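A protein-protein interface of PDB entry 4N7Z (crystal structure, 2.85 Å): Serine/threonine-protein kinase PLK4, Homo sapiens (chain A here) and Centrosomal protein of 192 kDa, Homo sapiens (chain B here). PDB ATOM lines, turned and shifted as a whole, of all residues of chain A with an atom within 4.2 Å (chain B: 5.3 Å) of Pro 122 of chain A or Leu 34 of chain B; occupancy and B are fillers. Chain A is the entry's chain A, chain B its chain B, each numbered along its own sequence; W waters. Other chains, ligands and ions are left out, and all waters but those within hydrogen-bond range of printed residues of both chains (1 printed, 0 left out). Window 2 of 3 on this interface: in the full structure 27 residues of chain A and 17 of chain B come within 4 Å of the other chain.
Leu 34 of chain B touches Lys 21 of chain A. Phe 31 of chain B touches Lys 120 of chain A (CD2 to CD, 3.4 Å). Lys 120 of chain A touches Leu 34 of chain B (O to CD1, 3.8 Å). Leu 34 of chain B touches Ser 121 of chain A. Leu 34 of chain B touches Pro 122 of chain A (O to CG, 3.8 Å).
The backbone NH (N) of Glu 137 of chain A sits close to the backbone carbonyl oxygen (O) of Ser 121 of chain A, at 3.2 Å.
Of the 11 printed residues of chain A, 4 touch a printed residue of chain B. Along chain A the printed residues that touch a printed residue of chain B span positions 21 to 122. Along chain B the printed residues that touch a printed residue of chain A span positions 30 to 34. Among the printed residues, 6 pairs touch across the chains. Among the printed residues, no Asp or Glu carboxylate lies within 4 Å of a Lys or Arg side-chain nitrogen of the other chain.
Of the printed residues of chain B, Lys 120 of chain A touches Phe 31 (3.4 Å) and Leu 34 (3.8 Å). Of the printed residues of chain B, Ser 121 of chain A touches Leu 34 (3.8 Å). Of the printed residues of chain B, Pro 122 of chain A touches Leu 34 (3.8 Å). Leu 34 of chain B touches just these residues of chain A: Lys 21 (3.8 Å), Lys 120 (3.8 Å), Ser 121 (3.8 Å) and Pro 122 (3.8 Å). The nearest residue of chain B that does not touch Pro 122 of chain A is Ala 35 of chain B (4.5 Å). The nearest printed residue of chain A that does not touch Leu 34 of chain B is Pro 221 of chain A (6.9 Å). The nearest printed residue of chain A that does not touch Phe 31 of chain B is Ser 121 of chain A (5.9 Å).
Water W1 lies within hydrogen-bond range of the side-chain hydroxyl of Ser 121 of chain A (2.7 Å), the backbone NH of Lys 21 of chain A (3.0 Å) and the side-chain hydroxyl of Tyr 30 of chain B (3.3 Å).
The backbone carbonyl oxygen (O) of Lys 21 of chain A is in hydrogen-bond range of the side-chain hydroxyl (OH) of Tyr 30 of chain B (2.7 Å).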
ATOM      1  N   LYS A  21       7.615 -10.445 -11.911  1.00  0.00           N
ATOM      2  CA  LYS A  21       7.096 -11.271 -13.018  1.00  0.00           C
ATOM      3  C   LYS A  21       5.670 -10.884 -13.419  1.00  0.00           C
ATOM      4  O   LYS A  21       4.857 -10.537 -12.567  1.00  0.00           O
ATOM      5  CB  LYS A  21       7.140 -12.750 -12.626  1.00  0.00           C
ATOM      6  CG  LYS A  21       7.017 -13.758 -13.782  1.00  0.00           C
ATOM      7  CD  LYS A  21       7.216 -15.189 -13.260  1.00  0.00           C
ATOM      8  CE  LYS A  21       6.822 -16.260 -14.270  1.00  0.00           C
ATOM      9  NZ  LYS A  21       7.919 -16.658 -15.209  1.00  0.00           N
ATOM     10  N   LYS A 120       6.143 -11.810  -1.833  1.00  0.00           N
ATOM     11  CA  LYS A 120       6.295 -13.190  -2.187  1.00  0.00           C
ATOM     12  C   LYS A 120       7.272 -13.424  -3.304  1.00  0.00           C
ATOM     13  O   LYS A 120       7.506 -14.520  -3.649  1.00  0.00           O
ATOM     14  CB  LYS A 120       4.931 -13.822  -2.507  1.00  0.00           C
ATOM     15  CG  LYS A 120       3.935 -13.787  -1.376  1.00  0.00           C
ATOM     16  CD  LYS A 120       3.218 -15.084  -1.186  1.00  0.00           C
ATOM     17  CE  LYS A 120       3.325 -15.590   0.216  1.00  0.00           C
ATOM     18  NZ  LYS A 120       2.164 -16.398   0.589  1.00  0.00           N
ATOM     19  N   SER A 121       7.854 -12.369  -3.840  1.00  0.00           N
ATOM     20  CA  SER A 121       8.854 -12.427  -4.915  1.00  0.00           C
ATOM     21  C   SER A 121      10.270 -12.438  -4.362  1.00  0.00           C
ATOM     22  O   SER A 121      10.773 -11.387  -3.970  1.00  0.00           O
ATOM     23  CB  SER A 121       8.753 -11.170  -5.771  1.00  0.00           C
ATOM     24  OG  SER A 121       7.502 -11.044  -6.399  1.00  0.00           O
ATOM     25  N   PRO A 122      10.935 -13.612  -4.347  1.00  0.00           N
ATOM     26  CA  PRO A 122      12.293 -13.678  -3.782  1.00  0.00           C
ATOM     27  C   PRO A 122      13.225 -12.629  -4.417  1.00  0.00           C
ATOM     28  O   PRO A 122      13.078 -12.333  -5.606  1.00  0.00           O
ATOM     29  CB  PRO A 122      12.744 -15.093  -4.158  1.00  0.00           C
ATOM     30  CG  PRO A 122      11.513 -15.847  -4.340  1.00  0.00           C
ATOM     31  CD  PRO A 122      10.531 -14.903  -4.935  1.00  0.00           C
ATOM     32  N   LYS A 123      14.129 -12.036  -3.638  1.00  0.00           N
ATOM     33  CA  LYS A 123      15.062 -11.048  -4.193  1.00  0.00           C
ATOM     34  C   LYS A 123      16.489 -11.567  -4.088  1.00  0.00           C
ATOM     35  O   LYS A 123      17.249 -11.558  -5.051  1.00  0.00           O
ATOM     36  CB  LYS A 123      14.932  -9.686  -3.504  1.00  0.00           C
ATOM     37  CG  LYS A 123      15.793  -8.605  -4.186  1.00  0.00           C
ATOM     38  CD  LYS A 123      15.514  -7.206  -3.655  1.00  0.00           C
ATOM     39  CE  LYS A 123      16.419  -6.152  -4.284  1.00  0.00           C
ATOM     40  NZ  LYS A 123      16.037  -4.730  -3.934  1.00  0.00           N
ATOM     41  N   ILE A 124      16.831 -12.036  -2.903  1.00  0.00           N
ATOM     42  CA  ILE A 124      18.090 -12.703  -2.700  1.00  0.00           C
ATOM     43  C   ILE A 124      17.834 -14.027  -2.003  1.00  0.00           C
ATOM     44  O   ILE A 124      17.283 -14.044  -0.897  1.00  0.00           O
ATOM     45  CB  ILE A 124      19.032 -11.875  -1.823  1.00  0.00           C
ATOM     46  CG1 ILE A 124      19.161 -10.440  -2.360  1.00  0.00           C
ATOM     47  CG2 ILE A 124      20.383 -12.563  -1.725  1.00  0.00           C
ATOM     48  CD1 ILE A 124      20.138  -9.594  -1.591  1.00  0.00           C
ATOM     49  N   ILE A 134      15.799 -16.429   2.349  1.00  0.00           N
ATOM     50  CA  ILE A 134      15.255 -15.698   1.194  1.00  0.00           C
ATOM     51  C   ILE A 134      14.786 -14.275   1.528  1.00  0.00           C
ATOM     52  O   ILE A 134      13.690 -14.111   2.067  1.00  0.00           O
ATOM     53  CB  ILE A 134      14.019 -16.408   0.600  1.00  0.00           C
ATOM     54  CG1 ILE A 134      14.244 -17.909   0.454  1.00  0.00           C
ATOM     55  CG2 ILE A 134      13.602 -15.767  -0.712  1.00  0.00           C
ATOM     56  CD1 ILE A 134      13.104 -18.605  -0.197  1.00  0.00           C
ATOM     57  N   LEU A 135      15.574 -13.250   1.194  1.00  0.00           N
ATOM     58  CA  LEU A 135      15.108 -11.874   1.357  1.00  0.00           C
ATOM     59  C   LEU A 135      14.112 -11.585   0.254  1.00  0.00           C
ATOM     60  O   LEU A 135      14.451 -11.710  -0.919  1.00  0.00           O
ATOM     61  CB  LEU A 135      16.268 -10.865   1.292  1.00  0.00           C
ATOM     62  CG  LEU A 135      15.976  -9.348   1.382  1.00  0.00           C
ATOM     63  CD1 LEU A 135      15.369  -8.961   2.726  1.00  0.00           C
ATOM     64  CD2 LEU A 135      17.212  -8.473   1.112  1.00  0.00           C
ATOM     65  N   MET A 136      12.887 -11.200   0.615  1.00  0.00           N
ATOM     66  CA  MET A 136      11.886 -10.865  -0.395  1.00  0.00           C
ATOM     67  C   MET A 136      12.011  -9.420  -0.903  1.00  0.00           C
ATOM     68  O   MET A 136      12.860  -8.652  -0.425  1.00  0.00           O
ATOM     69  CB  MET A 136      10.487 -11.140   0.136  1.00  0.00           C
ATOM     70  CG  MET A 136      10.296 -12.552   0.629  1.00  0.00           C
ATOM     71  SD  MET A 136      10.237 -13.774  -0.700  1.00  0.00           S
ATOM     72  CE  MET A 136      10.249 -15.267   0.308  1.00  0.00           C
ATOM     73  N   GLU A 137      11.165  -9.055  -1.864  1.00  0.00           N
ATOM     74  CA  GLU A 137      11.213  -7.732  -2.505  1.00  0.00           C
ATOM     75  C   GLU A 137      10.439  -6.595  -1.814  1.00  0.00           C
ATOM     76  O   GLU A 137      10.517  -5.444  -2.251  1.00  0.00           O
ATOM     77  CB  GLU A 137      10.716  -7.843  -3.952  1.00  0.00           C
ATOM     78  CG  GLU A 137      11.677  -8.509  -4.925  1.00  0.00           C
ATOM     79  CD  GLU A 137      12.540  -7.514  -5.676  1.00  0.00           C
ATOM     80  OE1 GLU A 137      13.367  -7.951  -6.506  1.00  0.00           O
ATOM     81  OE2 GLU A 137      12.391  -6.298  -5.441  1.00  0.00           O
ATOM     82  N   PRO A 221      16.133 -10.944  -9.631  1.00  0.00           N
ATOM     83  CA  PRO A 221      16.419 -11.903  -8.541  1.00  0.00           C
ATOM     84  C   PRO A 221      17.849 -12.448  -8.543  1.00  0.00           C
ATOM     85  O   PRO A 221      18.578 -12.297  -9.522  1.00  0.00           O
ATOM     86  CB  PRO A 221      15.402 -13.036  -8.777  1.00  0.00           C
ATOM     87  CG  PRO A 221      15.020 -12.931 -10.211  1.00  0.00           C
ATOM     88  CD  PRO A 221      15.130 -11.471 -10.578  1.00  0.00           C
ATOM     89  N   TYR B  30       1.293 -18.901  -9.102  1.00  0.00           N
ATOM     90  CA  TYR B  30       2.242 -17.947  -9.581  1.00  0.00           C
ATOM     91  C   TYR B  30       3.285 -17.799  -8.514  1.00  0.00           C
ATOM     92  O   TYR B  30       4.464 -17.855  -8.760  1.00  0.00           O
ATOM     93  CB  TYR B  30       1.496 -16.648  -9.835  1.00  0.00           C
ATOM     94  CG  TYR B  30       2.296 -15.375  -9.972  1.00  0.00           C
ATOM     95  CD1 TYR B  30       2.796 -14.977 -11.164  1.00  0.00           C
ATOM     96  CD2 TYR B  30       2.493 -14.556  -8.912  1.00  0.00           C
ATOM     97  CE1 TYR B  30       3.494 -13.825 -11.273  1.00  0.00           C
ATOM     98  CE2 TYR B  30       3.189 -13.409  -9.033  1.00  0.00           C
ATOM     99  CZ  TYR B  30       3.676 -13.066 -10.218  1.00  0.00           C
ATOM    100  OH  TYR B  30       4.351 -11.929 -10.322  1.00  0.00           O
ATOM    101  N   PHE B  31       2.824 -17.709  -7.294  1.00  0.00           N
ATOM    102  CA  PHE B  31       3.699 -17.559  -6.191  1.00  0.00           C
ATOM    103  C   PHE B  31       4.548 -18.789  -6.156  1.00  0.00           C
ATOM    104  O   PHE B  31       5.699 -18.731  -5.848  1.00  0.00           O
ATOM    105  CB  PHE B  31       2.924 -17.338  -4.918  1.00  0.00           C
ATOM    106  CG  PHE B  31       2.341 -15.975  -4.806  1.00  0.00           C
ATOM    107  CD1 PHE B  31       2.831 -14.925  -5.537  1.00  0.00           C
ATOM    108  CD2 PHE B  31       1.302 -15.735  -3.965  1.00  0.00           C
ATOM    109  CE1 PHE B  31       2.289 -13.672  -5.434  1.00  0.00           C
ATOM    110  CE2 PHE B  31       0.769 -14.482  -3.854  1.00  0.00           C
ATOM    111  CZ  PHE B  31       1.262 -13.452  -4.588  1.00  0.00           C
ATOM    112  N   GLU B  32       3.956 -19.908  -6.505  1.00  0.00           N
ATOM    113  CA  GLU B  32       4.666 -21.154  -6.500  1.00  0.00           C
ATOM    114  C   GLU B  32       5.814 -20.956  -7.390  1.00  0.00           C
ATOM    115  O   GLU B  32       6.886 -21.346  -7.083  1.00  0.00           O
ATOM    116  CB  GLU B  32       3.838 -22.251  -7.140  1.00  0.00           C
ATOM    117  CG  GLU B  32       2.755 -22.876  -6.294  1.00  0.00           C
ATOM    118  CD  GLU B  32       3.188 -23.152  -4.894  1.00  0.00           C
ATOM    119  OE1 GLU B  32       2.305 -23.428  -4.063  1.00  0.00           O
ATOM    120  OE2 GLU B  32       4.393 -23.088  -4.630  1.00  0.00           O
ATOM    121  N   GLN B  33       5.562 -20.378  -8.542  1.00  0.00           N
ATOM    122  CA  GLN B  33       6.528 -20.377  -9.607  1.00  0.00           C
ATOM    123  C   GLN B  33       7.790 -19.651  -9.264  1.00  0.00           C
ATOM    124  O   GLN B  33       8.839 -20.005  -9.724  1.00  0.00           O
ATOM    125  CB  GLN B  33       5.926 -19.824 -10.875  1.00  0.00           C
ATOM    126  CG  GLN B  33       4.819 -20.673 -11.444  1.00  0.00           C
ATOM    127  CD  GLN B  33       5.325 -21.858 -12.234  1.00  0.00           C
ATOM    128  OE1 GLN B  33       6.183 -21.722 -13.089  1.00  0.00           O
ATOM    129  NE2 GLN B  33       4.781 -23.027 -11.958  1.00  0.00           N
ATOM    130  N   LEU B  34       7.651 -18.575  -8.516  1.00  0.00           N
ATOM    131  CA  LEU B  34       8.732 -17.701  -8.144  1.00  0.00           C
ATOM    132  C   LEU B  34       9.740 -18.375  -7.275  1.00  0.00           C
ATOM    133  O   LEU B  34      10.897 -18.078  -7.323  1.00  0.00           O
ATOM    134  CB  LEU B  34       8.188 -16.454  -7.495  1.00  0.00           C
ATOM    135  CG  LEU B  34       7.057 -15.714  -8.183  1.00  0.00           C
ATOM    136  CD1 LEU B  34       6.520 -14.659  -7.269  1.00  0.00           C
ATOM    137  CD2 LEU B  34       7.507 -15.070  -9.449  1.00  0.00           C
ATOM    138  N   ALA B  35       9.273 -19.249  -6.425  1.00  0.00           N
ATOM    139  CA  ALA B  35      10.122 -19.929  -5.510  1.00  0.00           C
ATOM    140  C   ALA B  35      10.759 -21.139  -6.111  1.00  0.00           C
ATOM    141  O   ALA B  35      11.562 -21.777  -5.489  1.00  0.00           O
ATOM    142  CB  ALA B  35       9.328 -20.327  -4.317  1.00  0.00           C
ATOM    143  N   ILE B  36      10.355 -21.471  -7.313  1.00  0.00           N
ATOM    144  CA  ILE B  36      10.780 -22.683  -7.964  1.00  0.00           C
ATOM    145  C   ILE B  36      12.262 -22.669  -8.236  1.00  0.00           C
ATOM    146  O   ILE B  36      12.957 -23.651  -8.046  1.00  0.00           O
ATOM    147  CB  ILE B  36       9.866 -22.962  -9.174  1.00  0.00           C
ATOM    148  CG1 ILE B  36       9.031 -24.187  -8.915  1.00  0.00           C
ATOM    149  CG2 ILE B  36      10.589 -23.167 -10.483  1.00  0.00           C
ATOM    150  CD1 ILE B  36       7.754 -24.171  -9.696  1.00  0.00           C
ATOM    151  N   PRO B  37      12.752 -21.519  -8.619  1.00  0.00           N
ATOM    152  CA  PRO B  37      14.147 -21.365  -8.937  1.00  0.00           C
ATOM    153  C   PRO B  37      15.093 -21.690  -7.809  1.00  0.00           C
ATOM    154  O   PRO B  37      16.018 -22.345  -8.084  1.00  0.00           O
ATOM    155  CB  PRO B  37      14.214 -19.930  -9.334  1.00  0.00           C
ATOM    156  CG  PRO B  37      12.969 -19.755 -10.058  1.00  0.00           C
ATOM    157  CD  PRO B  37      11.951 -20.552  -9.350  1.00  0.00           C
ATOM    158  N   GLY B  38      14.864 -21.278  -6.588  1.00  0.00           N
ATOM    159  CA  GLY B  38      15.702 -21.677  -5.486  1.00  0.00           C
ATOM    160  C   GLY B  38      15.544 -23.131  -5.151  1.00  0.00           C
ATOM    161  O   GLY B  38      16.123 -23.658  -4.241  1.00  0.00           O
HETATM  162  O   HOH W   1       7.389 -11.379  -9.085  1.00  0.00           O
